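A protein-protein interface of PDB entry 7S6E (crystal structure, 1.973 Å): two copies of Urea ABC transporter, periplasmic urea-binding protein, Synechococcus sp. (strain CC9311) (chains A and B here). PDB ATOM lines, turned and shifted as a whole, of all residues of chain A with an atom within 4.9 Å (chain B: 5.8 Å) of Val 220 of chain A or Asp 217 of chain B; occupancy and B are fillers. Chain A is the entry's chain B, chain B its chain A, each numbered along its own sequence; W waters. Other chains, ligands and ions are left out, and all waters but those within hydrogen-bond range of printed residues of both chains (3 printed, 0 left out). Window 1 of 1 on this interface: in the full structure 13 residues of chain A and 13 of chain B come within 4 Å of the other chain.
Water W2 lies within hydrogen-bond range of the side-chain carboxylate of Asp 217 of chain B (2.6 Å), the backbone carbonyl oxygen of Gly 189 of chain B (2.6 Å) and the side-chain amino group of Lys 224 of chain A (2.9 Å).
Water W1 lies within hydrogen-bond range of the side-chain amino group of Lys 224 of chain A (2.7 Å), the side-chain carboxylate of Asp 217 of chain B (2.8 Å) and the backbone NH of Thr 21 of chain B (3.3 Å).
Water W3 lies within hydrogen-bond range of the backbone NH (N) of Thr 21 of chain B and the side-chain amino group (NZ) of Lys 224 of chain A.
Val 220 of chain A touches one residue of chain B.
Printed residues of chain A within 4 Å of Asp 217 of chain B: Val 220.
Of the printed residues of chain A, Thr 21 of chain B touches Lys 224.
Of the printed residues of chain B, Lys 224 of chain A touches Thr 21 (3.8 Å).
Of the printed residues of chain A, Thr 191 of chain B touches Ala 221.
Printed residues of chain B within 4 Å of Ala 221 of chain A: Thr 191.
The nearest printed residue of chain B that does not touch Lys 224 of chain A is Gly 189 of chain B (4.01 Å).
OD2 of Asp 217 of chain B touches CG1 of Val 220 of chain A (3.98 Å).
CB of Ala 221 of chain A touches OG1 of Thr 191 of chain B, at 3.2 Å.
Thr 21 of chain B touches Lys 224 of chain A.
Val 220 of chain A touches Asp 217 of chain B, but with the chains exchanged Asp 217 of chain A does not touch Val 220 of chain B (4.1 Å).
7 positions are printed for both chains.
Of the 3 pairs that touch across the chains among the printed residues, none has its exchanged pair printed and touching as well.
Of the 13 printed residues of chain B, 3 touch a printed residue of chain A.
Among the printed residues, 3 pairs touch across the chains.
OG1 of Thr 21 of chain B lies within hydrogen-bond range of OD1 of Asp 217 of chain B, 2.6 Å away.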
ATOM      1  N   ILE A  24      18.920  33.155  22.596  1.00  0.00           N
ATOM      2  CA  ILE A  24      20.069  33.022  23.538  1.00  0.00           C
ATOM      3  C   ILE A  24      21.107  34.150  23.300  1.00  0.00           C
ATOM      4  O   ILE A  24      21.777  34.618  24.284  1.00  0.00           O
ATOM      5  CB  ILE A  24      20.716  31.612  23.426  1.00  0.00           C
ATOM      6  CG1 ILE A  24      21.755  31.405  24.518  1.00  0.00           C
ATOM      7  CG2 ILE A  24      21.362  31.391  22.054  1.00  0.00           C
ATOM      8  CD1 ILE A  24      22.335  29.996  24.582  1.00  0.00           C
ATOM      9  N   GLY A 216      23.826  30.480  17.862  1.00  0.00           N
ATOM     10  CA  GLY A 216      22.560  30.229  18.573  1.00  0.00           C
ATOM     11  C   GLY A 216      22.661  29.063  19.534  1.00  0.00           C
ATOM     12  O   GLY A 216      23.812  28.634  19.896  1.00  0.00           O
ATOM     13  N   ASP A 217      21.522  28.553  20.006  1.00  0.00           N
ATOM     14  CA  ASP A 217      21.535  27.668  21.199  1.00  0.00           C
ATOM     15  C   ASP A 217      22.044  26.240  20.878  1.00  0.00           C
ATOM     16  O   ASP A 217      22.249  25.469  21.858  1.00  0.00           O
ATOM     17  CB  ASP A 217      20.184  27.712  21.925  1.00  0.00           C
ATOM     18  CG  ASP A 217      18.969  27.278  21.139  1.00  0.00           C
ATOM     19  OD1 ASP A 217      19.139  26.543  20.100  1.00  0.00           O
ATOM     20  OD2 ASP A 217      17.840  27.705  21.575  1.00  0.00           O
ATOM     21  N   GLN A 218      22.297  25.882  19.616  1.00  0.00           N
ATOM     22  CA  GLN A 218      22.949  24.560  19.332  1.00  0.00           C
ATOM     23  C   GLN A 218      24.335  24.524  19.989  1.00  0.00           C
ATOM     24  O   GLN A 218      24.863  23.428  20.192  1.00  0.00           O
ATOM     25  CB  GLN A 218      22.976  24.231  17.837  1.00  0.00           C
ATOM     26  CG  GLN A 218      23.934  25.050  16.993  1.00  0.00           C
ATOM     27  CD  GLN A 218      23.619  24.892  15.523  1.00  0.00           C
ATOM     28  OE1 GLN A 218      23.742  25.829  14.728  1.00  0.00           O
ATOM     29  NE2 GLN A 218      23.207  23.694  15.146  1.00  0.00           N
ATOM     30  N   ASN A 219      24.924  25.677  20.292  1.00  0.00           N
ATOM     31  CA  ASN A 219      26.197  25.766  21.045  1.00  0.00           C
ATOM     32  C   ASN A 219      26.092  25.049  22.397  1.00  0.00           C
ATOM     33  O   ASN A 219      27.126  24.558  22.895  1.00  0.00           O
ATOM     34  CB  ASN A 219      26.628  27.212  21.246  1.00  0.00           C
ATOM     35  CG  ASN A 219      27.373  27.751  20.048  1.00  0.00           C
ATOM     36  OD1 ASN A 219      28.548  27.444  19.837  1.00  0.00           O
ATOM     37  ND2 ASN A 219      26.676  28.539  19.262  1.00  0.00           N
ATOM     38  N   VAL A 220      24.914  25.030  22.987  1.00  0.00           N
ATOM     39  CA  VAL A 220      24.739  24.469  24.345  1.00  0.00           C
ATOM     40  C   VAL A 220      25.054  22.960  24.232  1.00  0.00           C
ATOM     41  O   VAL A 220      25.979  22.489  24.930  1.00  0.00           O
ATOM     42  CB  VAL A 220      23.339  24.777  24.900  1.00  0.00           C
ATOM     43  CG1 VAL A 220      23.154  24.122  26.262  1.00  0.00           C
ATOM     44  CG2 VAL A 220      23.057  26.279  24.977  1.00  0.00           C
ATOM     45  N   ALA A 221      24.359  22.251  23.347  1.00  0.00           N
ATOM     46  CA  ALA A 221      24.562  20.792  23.140  1.00  0.00           C
ATOM     47  C   ALA A 221      26.029  20.533  22.767  1.00  0.00           C
ATOM     48  O   ALA A 221      26.648  19.628  23.366  1.00  0.00           O
ATOM     49  CB  ALA A 221      23.629  20.317  22.083  1.00  0.00           C
ATOM     50  N   PHE A 222      26.587  21.362  21.873  1.00  0.00           N
ATOM     51  CA  PHE A 222      27.966  21.192  21.388  1.00  0.00           C
ATOM     52  C   PHE A 222      28.907  21.154  22.572  1.00  0.00           C
ATOM     53  O   PHE A 222      29.667  20.201  22.688  1.00  0.00           O
ATOM     54  CB  PHE A 222      28.376  22.275  20.393  1.00  0.00           C
ATOM     55  CG  PHE A 222      29.762  22.071  19.828  1.00  0.00           C
ATOM     56  CD1 PHE A 222      30.026  20.975  19.014  1.00  0.00           C
ATOM     57  CD2 PHE A 222      30.796  22.952  20.113  1.00  0.00           C
ATOM     58  CE1 PHE A 222      31.294  20.788  18.481  1.00  0.00           C
ATOM     59  CE2 PHE A 222      32.078  22.738  19.608  1.00  0.00           C
ATOM     60  CZ  PHE A 222      32.317  21.647  18.810  1.00  0.00           C
ATOM     61  N   PHE A 223      28.973  22.222  23.369  1.00  0.00           N
ATOM     62  CA  PHE A 223      30.005  22.319  24.430  1.00  0.00           C
ATOM     63  C   PHE A 223      29.760  21.249  25.496  1.00  0.00           C
ATOM     64  O   PHE A 223      30.743  20.753  26.044  1.00  0.00           O
ATOM     65  CB  PHE A 223      30.123  23.744  24.992  1.00  0.00           C
ATOM     66  CG  PHE A 223      30.930  24.638  24.081  1.00  0.00           C
ATOM     67  CD1 PHE A 223      32.307  24.558  24.060  1.00  0.00           C
ATOM     68  CD2 PHE A 223      30.301  25.466  23.161  1.00  0.00           C
ATOM     69  CE1 PHE A 223      33.030  25.327  23.169  1.00  0.00           C
ATOM     70  CE2 PHE A 223      31.037  26.245  22.278  1.00  0.00           C
ATOM     71  CZ  PHE A 223      32.397  26.181  22.290  1.00  0.00           C
ATOM     72  N   LYS A 224      28.510  20.905  25.789  1.00  0.00           N
ATOM     73  CA  LYS A 224      28.256  19.854  26.824  1.00  0.00           C
ATOM     74  C   LYS A 224      28.723  18.488  26.303  1.00  0.00           C
ATOM     75  O   LYS A 224      29.353  17.755  27.077  1.00  0.00           O
ATOM     76  CB  LYS A 224      26.802  19.886  27.290  1.00  0.00           C
ATOM     77  CG  LYS A 224      26.541  21.168  28.090  1.00  0.00           C
ATOM     78  CD  LYS A 224      25.119  21.376  28.562  1.00  0.00           C
ATOM     79  CE  LYS A 224      25.038  22.624  29.445  1.00  0.00           C
ATOM     80  NZ  LYS A 224      23.631  23.025  29.686  1.00  0.00           N
ATOM     81  N   ILE A 252      25.396  28.802  28.888  1.00  0.00           N
ATOM     82  CA  ILE A 252      25.847  27.386  28.722  1.00  0.00           C
ATOM     83  C   ILE A 252      26.349  26.861  30.062  1.00  0.00           C
ATOM     84  O   ILE A 252      26.091  25.669  30.368  1.00  0.00           O
ATOM     85  CB  ILE A 252      26.947  27.267  27.651  1.00  0.00           C
ATOM     86  CG1 ILE A 252      26.391  27.552  26.267  1.00  0.00           C
ATOM     87  CG2 ILE A 252      27.602  25.894  27.684  1.00  0.00           C
ATOM     88  CD1 ILE A 252      27.446  28.001  25.281  1.00  0.00           C
ATOM     89  N   GLY B  20      23.143  28.363  33.314  1.00  0.00           N
ATOM     90  CA  GLY B  20      23.054  26.896  33.113  1.00  0.00           C
ATOM     91  C   GLY B  20      21.703  26.462  32.546  1.00  0.00           C
ATOM     92  O   GLY B  20      20.840  27.311  32.228  1.00  0.00           O
ATOM     93  N   THR B  21      21.490  25.155  32.485  1.00  0.00           N
ATOM     94  CA  THR B  21      20.347  24.486  31.815  1.00  0.00           C
ATOM     95  C   THR B  21      18.973  24.954  32.363  1.00  0.00           C
ATOM     96  O   THR B  21      18.013  24.889  31.606  1.00  0.00           O
ATOM     97  CB  THR B  21      20.523  22.955  31.880  1.00  0.00           C
ATOM     98  OG1 THR B  21      19.527  22.427  30.999  1.00  0.00           O
ATOM     99  CG2 THR B  21      20.478  22.427  33.308  1.00  0.00           C
ATOM    100  N   MET B  22      18.866  25.449  33.606  1.00  0.00           N
ATOM    101  CA  MET B  22      17.546  25.824  34.190  1.00  0.00           C
ATOM    102  C   MET B  22      17.242  27.317  33.941  1.00  0.00           C
ATOM    103  O   MET B  22      16.105  27.755  34.217  1.00  0.00           O
ATOM    104  CB  MET B  22      17.484  25.500  35.696  1.00  0.00           C
ATOM    105  CG  MET B  22      17.503  23.989  35.991  1.00  0.00           C
ATOM    106  SD  MET B  22      16.281  23.058  35.087  1.00  0.00           S
ATOM    107  CE  MET B  22      14.774  23.940  35.495  1.00  0.00           C
ATOM    108  N   ILE B  24      16.655  28.939  31.238  1.00  0.00           N
ATOM    109  CA  ILE B  24      15.508  29.050  30.276  1.00  0.00           C
ATOM    110  C   ILE B  24      14.160  29.142  31.026  1.00  0.00           C
ATOM    111  O   ILE B  24      13.214  29.786  30.516  1.00  0.00           O
ATOM    112  CB  ILE B  24      15.500  27.850  29.296  1.00  0.00           C
ATOM    113  CG1 ILE B  24      14.492  28.061  28.172  1.00  0.00           C
ATOM    114  CG2 ILE B  24      15.231  26.539  30.017  1.00  0.00           C
ATOM    115  CD1 ILE B  24      14.446  26.919  27.149  1.00  0.00           C
ATOM    116  N   GLY B 189      20.054  18.537  31.264  1.00  0.00           N
ATOM    117  CA  GLY B 189      20.887  19.284  30.311  1.00  0.00           C
ATOM    118  C   GLY B 189      21.347  18.471  29.108  1.00  0.00           C
ATOM    119  O   GLY B 189      21.863  19.070  28.165  1.00  0.00           O
ATOM    120  N   THR B 191      21.265  16.364  25.701  1.00  0.00           N
ATOM    121  CA  THR B 191      20.495  16.535  24.433  1.00  0.00           C
ATOM    122  C   THR B 191      20.564  15.271  23.548  1.00  0.00           C
ATOM    123  O   THR B 191      20.024  15.305  22.417  1.00  0.00           O
ATOM    124  CB  THR B 191      20.986  17.799  23.694  1.00  0.00           C
ATOM    125  OG1 THR B 191      22.399  17.718  23.494  1.00  0.00           O
ATOM    126  CG2 THR B 191      20.675  19.079  24.458  1.00  0.00           C
ATOM    127  N   ASN B 215      13.073  18.747  32.374  1.00  0.00           N
ATOM    128  CA  ASN B 215      13.166  20.105  32.949  1.00  0.00           C
ATOM    129  C   ASN B 215      14.291  20.824  32.206  1.00  0.00           C
ATOM    130  O   ASN B 215      15.321  20.167  31.819  1.00  0.00           O
ATOM    131  CB  ASN B 215      13.360  20.069  34.462  1.00  0.00           C
ATOM    132  CG  ASN B 215      12.061  19.932  35.242  1.00  0.00           C
ATOM    133  OD1 ASN B 215      11.651  20.828  35.974  1.00  0.00           O
ATOM    134  ND2 ASN B 215      11.347  18.833  35.045  1.00  0.00           N
ATOM    135  N   GLY B 216      14.150  22.133  32.080  1.00  0.00           N
ATOM    136  CA  GLY B 216      15.223  22.993  31.542  1.00  0.00           C
ATOM    137  C   GLY B 216      15.447  22.885  30.047  1.00  0.00           C
ATOM    138  O   GLY B 216      14.592  22.368  29.332  1.00  0.00           O
ATOM    139  N   ASP B 217      16.603  23.339  29.566  1.00  0.00           N
ATOM    140  CA  ASP B 217      16.807  23.603  28.120  1.00  0.00           C
ATOM    141  C   ASP B 217      16.961  22.313  27.303  1.00  0.00           C
ATOM    142  O   ASP B 217      16.926  22.442  26.080  1.00  0.00           O
ATOM    143  CB  ASP B 217      17.872  24.679  27.817  1.00  0.00           C
ATOM    144  CG  ASP B 217      19.300  24.409  28.227  1.00  0.00           C
ATOM    145  OD1 ASP B 217      19.573  23.190  28.511  1.00  0.00           O
ATOM    146  OD2 ASP B 217      20.096  25.473  28.420  1.00  0.00           O
ATOM    147  N   GLN B 218      16.987  21.125  27.903  1.00  0.00           N
ATOM    148  CA  GLN B 218      17.053  19.872  27.114  1.00  0.00           C
ATOM    149  C   GLN B 218      15.712  19.667  26.410  1.00  0.00           C
ATOM    150  O   GLN B 218      15.705  18.937  25.411  1.00  0.00           O
ATOM    151  CB  GLN B 218      17.465  18.674  27.965  1.00  0.00           C
ATOM    152  CG  GLN B 218      16.413  18.146  28.930  1.00  0.00           C
ATOM    153  CD  GLN B 218      16.992  17.184  29.942  1.00  0.00           C
ATOM    154  OE1 GLN B 218      16.686  17.257  31.125  1.00  0.00           O
ATOM    155  NE2 GLN B 218      17.853  16.285  29.487  1.00  0.00           N
ATOM    156  N   ASN B 219      14.639  20.349  26.849  1.00  0.00           N
ATOM    157  CA  ASN B 219      13.329  20.362  26.159  1.00  0.00           C
ATOM    158  C   ASN B 219      13.479  20.869  24.713  1.00  0.00           C
ATOM    159  O   ASN B 219      12.683  20.423  23.843  1.00  0.00           O
ATOM    160  CB  ASN B 219      12.268  21.162  26.903  1.00  0.00           C
ATOM    161  CG  ASN B 219      11.650  20.394  28.052  1.00  0.00           C
ATOM    162  OD1 ASN B 219      10.776  19.580  27.834  1.00  0.00           O
ATOM    163  ND2 ASN B 219      12.042  20.670  29.284  1.00  0.00           N
ATOM    164  N   VAL B 220      14.441  21.761  24.452  1.00  0.00           N
ATOM    165  CA  VAL B 220      14.584  22.375  23.106  1.00  0.00           C
ATOM    166  C   VAL B 220      14.894  21.227  22.114  1.00  0.00           C
ATOM    167  O   VAL B 220      14.146  21.057  21.145  1.00  0.00           O
ATOM    168  CB  VAL B 220      15.636  23.484  23.140  1.00  0.00           C
ATOM    169  CG1 VAL B 220      15.921  24.051  21.755  1.00  0.00           C
ATOM    170  CG2 VAL B 220      15.277  24.608  24.118  1.00  0.00           C
ATOM    171  N   ALA B 221      15.932  20.447  22.378  1.00  0.00           N
ATOM    172  CA  ALA B 221      16.350  19.320  21.520  1.00  0.00           C
ATOM    173  C   ALA B 221      15.204  18.305  21.457  1.00  0.00           C
ATOM    174  O   ALA B 221      14.874  17.795  20.365  1.00  0.00           O
ATOM    175  CB  ALA B 221      17.617  18.754  22.081  1.00  0.00           C
HETATM  176  O   HOH W   1      22.685  25.497  29.431  1.00  0.00           O
HETATM  177  O   HOH W   2      21.578  21.657  28.121  1.00  0.00           O
HETATM  178  O   HOH W   3      23.803  23.782  33.024  1.00  0.00           O
